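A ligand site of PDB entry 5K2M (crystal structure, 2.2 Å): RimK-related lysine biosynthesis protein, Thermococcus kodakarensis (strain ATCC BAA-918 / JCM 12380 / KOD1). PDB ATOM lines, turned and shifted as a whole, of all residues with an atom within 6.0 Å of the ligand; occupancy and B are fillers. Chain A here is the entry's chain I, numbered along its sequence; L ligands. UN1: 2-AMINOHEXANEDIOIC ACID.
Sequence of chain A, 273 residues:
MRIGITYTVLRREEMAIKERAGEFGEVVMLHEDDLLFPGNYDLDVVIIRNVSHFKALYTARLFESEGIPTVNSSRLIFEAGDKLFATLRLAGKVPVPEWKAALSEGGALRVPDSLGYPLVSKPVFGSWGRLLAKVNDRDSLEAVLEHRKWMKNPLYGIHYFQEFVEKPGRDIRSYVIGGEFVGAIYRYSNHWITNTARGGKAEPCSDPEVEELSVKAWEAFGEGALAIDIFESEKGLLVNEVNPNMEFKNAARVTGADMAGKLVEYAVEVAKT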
ATOM      1  N   GLU A  13       4.295  19.868 -17.838  1.00  0.00           N
ATOM      2  CA  GLU A  13       4.002  21.176 -18.450  1.00  0.00           C
ATOM      3  C   GLU A  13       3.037  22.030 -17.624  1.00  0.00           C
ATOM      4  O   GLU A  13       3.304  23.206 -17.409  1.00  0.00           O
ATOM      5  CB  GLU A  13       3.539  21.066 -19.925  1.00  0.00           C
ATOM      6  CG  GLU A  13       2.980  19.725 -20.389  1.00  0.00           C
ATOM      7  CD  GLU A  13       4.044  18.799 -20.944  1.00  0.00           C
ATOM      8  OE1 GLU A  13       4.648  19.141 -21.981  1.00  0.00           O
ATOM      9  OE2 GLU A  13       4.261  17.728 -20.343  1.00  0.00           O
ATOM     10  N   SER A 127      -3.477  13.123 -32.995  1.00  0.00           N
ATOM     11  CA  SER A 127      -2.179  13.569 -32.494  1.00  0.00           C
ATOM     12  C   SER A 127      -1.448  12.357 -31.911  1.00  0.00           C
ATOM     13  O   SER A 127      -2.069  11.329 -31.624  1.00  0.00           O
ATOM     14  CB  SER A 127      -2.349  14.648 -31.413  1.00  0.00           C
ATOM     15  OG  SER A 127      -1.098  15.193 -31.019  1.00  0.00           O
ATOM     16  N   TRP A 128      -0.116  12.459 -31.777  1.00  0.00           N
ATOM     17  CA  TRP A 128       0.712  11.514 -30.986  1.00  0.00           C
ATOM     18  C   TRP A 128       1.471  10.322 -31.654  1.00  0.00           C
ATOM     19  O   TRP A 128       2.261   9.682 -30.960  1.00  0.00           O
ATOM     20  CB  TRP A 128      -0.016  11.002 -29.717  1.00  0.00           C
ATOM     21  CG  TRP A 128      -0.010  11.957 -28.521  1.00  0.00           C
ATOM     22  CD1 TRP A 128       0.666  13.140 -28.410  1.00  0.00           C
ATOM     23  CD2 TRP A 128      -0.665  11.747 -27.253  1.00  0.00           C
ATOM     24  NE1 TRP A 128       0.446  13.693 -27.163  1.00  0.00           N
ATOM     25  CE2 TRP A 128      -0.366  12.869 -26.444  1.00  0.00           C
ATOM     26  CE3 TRP A 128      -1.497  10.739 -26.743  1.00  0.00           C
ATOM     27  CZ2 TRP A 128      -0.867  13.003 -25.136  1.00  0.00           C
ATOM     28  CZ3 TRP A 128      -1.990  10.881 -25.445  1.00  0.00           C
ATOM     29  CH2 TRP A 128      -1.660  12.003 -24.655  1.00  0.00           C
ATOM     30  N   ARG A 173      10.581  19.740 -34.816  1.00  0.00           N
ATOM     31  CA  ARG A 173       9.518  20.288 -33.989  1.00  0.00           C
ATOM     32  C   ARG A 173      10.007  21.622 -33.434  1.00  0.00           C
ATOM     33  O   ARG A 173      10.939  21.668 -32.624  1.00  0.00           O
ATOM     34  CB  ARG A 173       9.207  19.322 -32.857  1.00  0.00           C
ATOM     35  CG  ARG A 173       8.252  19.834 -31.806  1.00  0.00           C
ATOM     36  CD  ARG A 173       6.818  19.739 -32.279  1.00  0.00           C
ATOM     37  NE  ARG A 173       5.915  19.557 -31.141  1.00  0.00           N
ATOM     38  CZ  ARG A 173       4.664  19.123 -31.232  1.00  0.00           C
ATOM     39  NH1 ARG A 173       4.134  18.811 -32.398  1.00  0.00           N
ATOM     40  NH2 ARG A 173       3.938  18.996 -30.124  1.00  0.00           N
ATOM     41  N   TYR A 175       8.845  25.767 -31.985  1.00  0.00           N
ATOM     42  CA  TYR A 175       7.858  26.460 -31.172  1.00  0.00           C
ATOM     43  C   TYR A 175       7.866  27.956 -31.448  1.00  0.00           C
ATOM     44  O   TYR A 175       8.921  28.595 -31.418  1.00  0.00           O
ATOM     45  CB  TYR A 175       8.115  26.201 -29.689  1.00  0.00           C
ATOM     46  CG  TYR A 175       7.991  24.754 -29.297  1.00  0.00           C
ATOM     47  CD1 TYR A 175       9.006  23.859 -29.557  1.00  0.00           C
ATOM     48  CD2 TYR A 175       6.844  24.285 -28.675  1.00  0.00           C
ATOM     49  CE1 TYR A 175       8.897  22.530 -29.203  1.00  0.00           C
ATOM     50  CE2 TYR A 175       6.713  22.962 -28.321  1.00  0.00           C
ATOM     51  CZ  TYR A 175       7.745  22.082 -28.587  1.00  0.00           C
ATOM     52  OH  TYR A 175       7.636  20.753 -28.232  1.00  0.00           O
ATOM     53  N   ILE A 185      13.606  21.432 -31.915  1.00  0.00           N
ATOM     54  CA  ILE A 185      14.313  20.162 -31.699  1.00  0.00           C
ATOM     55  C   ILE A 185      14.206  19.244 -32.905  1.00  0.00           C
ATOM     56  O   ILE A 185      13.354  19.423 -33.764  1.00  0.00           O
ATOM     57  CB  ILE A 185      13.760  19.392 -30.470  1.00  0.00           C
ATOM     58  CG1 ILE A 185      12.277  19.059 -30.641  1.00  0.00           C
ATOM     59  CG2 ILE A 185      13.993  20.207 -29.199  1.00  0.00           C
ATOM     60  CD1 ILE A 185      11.740  18.096 -29.603  1.00  0.00           C
ATOM     61  N   ARG A 187      13.440  15.255 -33.794  1.00  0.00           N
ATOM     62  CA  ARG A 187      12.901  14.013 -33.251  1.00  0.00           C
ATOM     63  C   ARG A 187      13.389  12.832 -34.079  1.00  0.00           C
ATOM     64  O   ARG A 187      13.013  12.697 -35.241  1.00  0.00           O
ATOM     65  CB  ARG A 187      11.376  14.046 -33.231  1.00  0.00           C
ATOM     66  CG  ARG A 187      10.812  15.079 -32.277  1.00  0.00           C
ATOM     67  CD  ARG A 187       9.293  15.048 -32.253  1.00  0.00           C
ATOM     68  NE  ARG A 187       8.727  15.423 -33.543  1.00  0.00           N
ATOM     69  CZ  ARG A 187       7.447  15.717 -33.749  1.00  0.00           C
ATOM     70  NH1 ARG A 187       6.568  15.676 -32.750  1.00  0.00           N
ATOM     71  NH2 ARG A 187       7.031  16.046 -34.972  1.00  0.00           N
ATOM     72  N   THR A 194       7.672   9.639 -36.014  1.00  0.00           N
ATOM     73  CA  THR A 194       8.720  10.075 -35.090  1.00  0.00           C
ATOM     74  C   THR A 194       8.237  10.835 -33.836  1.00  0.00           C
ATOM     75  O   THR A 194       9.004  11.607 -33.260  1.00  0.00           O
ATOM     76  CB  THR A 194       9.737  11.000 -35.801  1.00  0.00           C
ATOM     77  OG1 THR A 194       9.137  12.292 -36.016  1.00  0.00           O
ATOM     78  CG2 THR A 194      10.201  10.428 -37.133  1.00  0.00           C
ATOM     79  N   ASN A 195       7.006  10.606 -33.387  1.00  0.00           N
ATOM     80  CA  ASN A 195       6.500  11.387 -32.236  1.00  0.00           C
ATOM     81  C   ASN A 195       7.212  10.971 -30.961  1.00  0.00           C
ATOM     82  O   ASN A 195       7.610   9.811 -30.830  1.00  0.00           O
ATOM     83  CB  ASN A 195       4.996  11.206 -32.044  1.00  0.00           C
ATOM     84  CG  ASN A 195       4.185  11.750 -33.198  1.00  0.00           C
ATOM     85  OD1 ASN A 195       3.456  12.726 -33.056  1.00  0.00           O
ATOM     86  ND2 ASN A 195       4.315  11.104 -34.334  1.00  0.00           N
ATOM     87  N   THR A 196       7.375  11.918 -30.037  1.00  0.00           N
ATOM     88  CA  THR A 196       7.962  11.601 -28.715  1.00  0.00           C
ATOM     89  C   THR A 196       6.975  10.813 -27.838  1.00  0.00           C
ATOM     90  O   THR A 196       7.396  10.036 -26.975  1.00  0.00           O
ATOM     91  CB  THR A 196       8.428  12.861 -27.945  1.00  0.00           C
ATOM     92  OG1 THR A 196       7.315  13.702 -27.653  1.00  0.00           O
ATOM     93  CG2 THR A 196       9.480  13.646 -28.748  1.00  0.00           C
ATOM     94  N   ALA A 197       5.666  11.000 -28.060  1.00  0.00           N
ATOM     95  CA  ALA A 197       4.633  10.169 -27.430  1.00  0.00           C
ATOM     96  C   ALA A 197       4.717   8.705 -27.888  1.00  0.00           C
ATOM     97  O   ALA A 197       4.304   7.802 -27.183  1.00  0.00           O
ATOM     98  CB  ALA A 197       3.241  10.716 -27.724  1.00  0.00           C
ATOM     99  N   ARG A 198       5.275   8.510 -29.091  1.00  0.00           N
ATOM    100  CA  ARG A 198       5.466   7.186 -29.671  1.00  0.00           C
ATOM    101  C   ARG A 198       6.850   6.591 -29.338  1.00  0.00           C
ATOM    102  O   ARG A 198       7.042   5.380 -29.436  1.00  0.00           O
ATOM    103  CB  ARG A 198       5.223   7.272 -31.193  1.00  0.00           C
ATOM    104  CG  ARG A 198       5.694   6.086 -32.016  1.00  0.00           C
ATOM    105  CD  ARG A 198       7.087   6.314 -32.603  1.00  0.00           C
ATOM    106  NE  ARG A 198       7.824   5.062 -32.801  1.00  0.00           N
ATOM    107  CZ  ARG A 198       7.518   4.134 -33.706  1.00  0.00           C
ATOM    108  NH1 ARG A 198       6.470   4.276 -34.514  1.00  0.00           N
ATOM    109  NH2 ARG A 198       8.275   3.040 -33.801  1.00  0.00           N
ATOM    110  N   ALA A 202      14.673  13.221 -28.530  1.00  0.00           N
ATOM    111  CA  ALA A 202      14.849  14.639 -28.837  1.00  0.00           C
ATOM    112  C   ALA A 202      16.315  15.083 -28.806  1.00  0.00           C
ATOM    113  O   ALA A 202      17.084  14.614 -27.964  1.00  0.00           O
ATOM    114  CB  ALA A 202      14.021  15.484 -27.879  1.00  0.00           C
ATOM    115  N   ASN A 245      -2.124  22.741 -29.006  1.00  0.00           N
ATOM    116  CA  ASN A 245      -2.119  22.243 -27.639  1.00  0.00           C
ATOM    117  C   ASN A 245      -0.731  21.665 -27.352  1.00  0.00           C
ATOM    118  O   ASN A 245      -0.565  20.468 -27.163  1.00  0.00           O
ATOM    119  CB  ASN A 245      -3.225  21.194 -27.470  1.00  0.00           C
ATOM    120  CG  ASN A 245      -4.604  21.708 -27.919  1.00  0.00           C
ATOM    121  OD1 ASN A 245      -5.043  22.788 -27.508  1.00  0.00           O
ATOM    122  ND2 ASN A 245      -5.279  20.925 -28.774  1.00  0.00           N
ATOM    123  N   MET A 246       0.255  22.561 -27.312  1.00  0.00           N
ATOM    124  CA  MET A 246       1.670  22.175 -27.328  1.00  0.00           C
ATOM    125  C   MET A 246       2.157  21.424 -26.083  1.00  0.00           C
ATOM    126  O   MET A 246       1.978  21.875 -24.944  1.00  0.00           O
ATOM    127  CB  MET A 246       2.559  23.415 -27.543  1.00  0.00           C
ATOM    128  CG  MET A 246       2.433  24.520 -26.513  1.00  0.00           C
ATOM    129  SD  MET A 246       3.735  25.778 -26.631  1.00  0.00           S
ATOM    130  CE  MET A 246       3.620  26.189 -28.367  1.00  0.00           C
ATOM    131  N   GLU A 247       2.747  20.263 -26.310  1.00  0.00           N
ATOM    132  CA  GLU A 247       3.581  19.621 -25.294  1.00  0.00           C
ATOM    133  C   GLU A 247       5.015  20.076 -25.558  1.00  0.00           C
ATOM    134  O   GLU A 247       5.406  20.303 -26.704  1.00  0.00           O
ATOM    135  CB  GLU A 247       3.462  18.102 -25.354  1.00  0.00           C
ATOM    136  CG  GLU A 247       2.116  17.573 -24.891  1.00  0.00           C
ATOM    137  CD  GLU A 247       2.120  16.069 -24.686  1.00  0.00           C
ATOM    138  OE1 GLU A 247       1.873  15.626 -23.545  1.00  0.00           O
ATOM    139  OE2 GLU A 247       2.395  15.321 -25.659  1.00  0.00           O
ATOM    140  N   PHE A 248       5.805  20.206 -24.495  1.00  0.00           N
ATOM    141  CA  PHE A 248       7.159  20.754 -24.624  1.00  0.00           C
ATOM    142  C   PHE A 248       8.192  20.299 -23.574  1.00  0.00           C
ATOM    143  O   PHE A 248       9.317  20.801 -23.587  1.00  0.00           O
ATOM    144  CB  PHE A 248       7.076  22.284 -24.591  1.00  0.00           C
ATOM    145  CG  PHE A 248       6.387  22.817 -23.377  1.00  0.00           C
ATOM    146  CD1 PHE A 248       7.073  22.954 -22.173  1.00  0.00           C
ATOM    147  CD2 PHE A 248       5.053  23.178 -23.420  1.00  0.00           C
ATOM    148  CE1 PHE A 248       6.438  23.446 -21.039  1.00  0.00           C
ATOM    149  CE2 PHE A 248       4.410  23.661 -22.299  1.00  0.00           C
ATOM    150  CZ  PHE A 248       5.094  23.808 -21.109  1.00  0.00           C
ATOM    151  N   LYS A 249       7.841  19.359 -22.689  1.00  0.00           N
ATOM    152  CA  LYS A 249       8.724  19.064 -21.559  1.00  0.00           C
ATOM    153  C   LYS A 249      10.079  18.521 -22.008  1.00  0.00           C
ATOM    154  O   LYS A 249      11.090  18.845 -21.382  1.00  0.00           O
ATOM    155  CB  LYS A 249       8.067  18.155 -20.508  1.00  0.00           C
ATOM    156  CG  LYS A 249       7.732  16.736 -20.932  1.00  0.00           C
ATOM    157  CD  LYS A 249       7.214  15.944 -19.738  1.00  0.00           C
ATOM    158  CE  LYS A 249       6.499  14.660 -20.138  1.00  0.00           C
ATOM    159  NZ  LYS A 249       7.384  13.729 -20.886  1.00  0.00           N
ATOM    160  N   ASN A 250      10.112  17.720 -23.071  1.00  0.00           N
ATOM    161  CA  ASN A 250      11.397  17.282 -23.649  1.00  0.00           C
ATOM    162  C   ASN A 250      12.083  18.407 -24.427  1.00  0.00           C
ATOM    163  O   ASN A 250      13.294  18.627 -24.270  1.00  0.00           O
ATOM    164  CB  ASN A 250      11.223  16.059 -24.549  1.00  0.00           C
ATOM    165  CG  ASN A 250      10.789  14.821 -23.803  1.00  0.00           C
ATOM    166  OD1 ASN A 250      11.364  14.469 -22.771  1.00  0.00           O
ATOM    167  ND2 ASN A 250       9.783  14.140 -24.315  1.00  0.00           N
ATOM    168  N   ALA A 251      11.312  19.106 -25.246  1.00  0.00           N
ATOM    169  CA  ALA A 251      11.825  20.259 -26.007  1.00  0.00           C
ATOM    170  C   ALA A 251      12.497  21.304 -25.113  1.00  0.00           C
ATOM    171  O   ALA A 251      13.542  21.829 -25.458  1.00  0.00           O
ATOM    172  CB  ALA A 251      10.713  20.896 -26.815  1.00  0.00           C
ATOM    173  N   ALA A 252      11.868  21.598 -23.973  1.00  0.00           N
ATOM    174  CA  ALA A 252      12.404  22.551 -22.990  1.00  0.00           C
ATOM    175  C   ALA A 252      13.660  22.022 -22.326  1.00  0.00           C
ATOM    176  O   ALA A 252      14.643  22.748 -22.201  1.00  0.00           O
ATOM    177  CB  ALA A 252      11.341  22.854 -21.938  1.00  0.00           C
HETATM  178  C1' UN1 L   1       8.336  17.142 -26.622  1.00  0.00           C
HETATM  179  O1' UN1 L   1       8.576  17.944 -25.691  1.00  0.00           O
HETATM  180  O2' UN1 L   1       8.445  15.906 -26.498  1.00  0.00           O
HETATM  181  O   UN1 L   1       4.032  13.644 -28.779  1.00  0.00           O
HETATM  182  C1  UN1 L   1       7.907  17.695 -27.961  1.00  0.00           C
HETATM  183  C   UN1 L   1       4.814  14.468 -29.300  1.00  0.00           C
HETATM  184  CA  UN1 L   1       4.621  15.929 -29.014  1.00  0.00           C
HETATM  185  C5  UN1 L   1       5.701  16.463 -28.061  1.00  0.00           C
HETATM  186  C6  UN1 L   1       7.026  16.733 -28.765  1.00  0.00           C
HETATM  187  N   UN1 L   1       3.311  16.157 -28.419  1.00  0.00           N
HETATM  188  OXT UN1 L   1       5.748  14.124 -30.069  1.00  0.00           O
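The backbone carbonyl oxygen of Glu 247 is in hydrogen-bond range of the side-chain hydroxyl of Tyr 175 (2.7 Å).
The side-chain carboxylate (OE2) of Glu 247 sits at hydrogen-bond distance from the indole nitrogen (NE1) of Trp 128, at 3.0 Å.
The backbone NH (N) of Phe 248 sits at hydrogen-bond distance from the side-chain carboxylate (OE1) of Glu 13 (3.0 Å).
The backbone carbonyl oxygen (O) of Arg 173 sits at hydrogen-bond distance from the backbone NH (N) of Ile 185, 2.8 Å away.
OE1 of Glu 13 is in hydrogen-bond range of N of Lys 249, at 3.3 Å.
Residues that only touch the ligand: Tyr 175 (3.1 Å), Phe 248 (3.2 Å), Trp 128 (3.4 Å) and Asn 195 (3.6 Å).
Hydrophobic or aromatic side chains that line the ligand: Trp 128, Ala 197 and Ala 251.
The backbone NH (N) of Thr 196 is in hydrogen-bond range of an oxygen (OXT) of the ligand, at 2.7 Å.
O2' of the ligand is in hydrogen-bond range of OG1 of Thr 196.
The backbone NH of Ala 251 sits at hydrogen-bond distance from an oxygen (O1') of the ligand.
OE2 of Glu 247 is in salt-bridge range of N of the ligand (3.0 Å).
An oxygen (O1') of the ligand is in hydrogen-bond range of the backbone NH (N) of Asn 250 (3.0 Å).
The side-chain amide nitrogen (ND2) of Asn 250 lies within hydrogen-bond range of an oxygen (O2') of the ligand (3.1 Å).
The backbone NH of Ala 197 lies within hydrogen-bond range of an oxygen (O) of the ligand (3.2 Å).
The guanidinium group (NH1) of Arg 187 lies within salt-bridge range of an oxygen (OXT) of the ligand (3.2 Å).
The guanidinium group (NH2) of Arg 173 lies close to a nitrogen (N) of the ligand, 3.4 Å away.
The backbone NH of Lys 249 lies within hydrogen-bond range of an oxygen (O1') of the ligand (3.4 Å).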
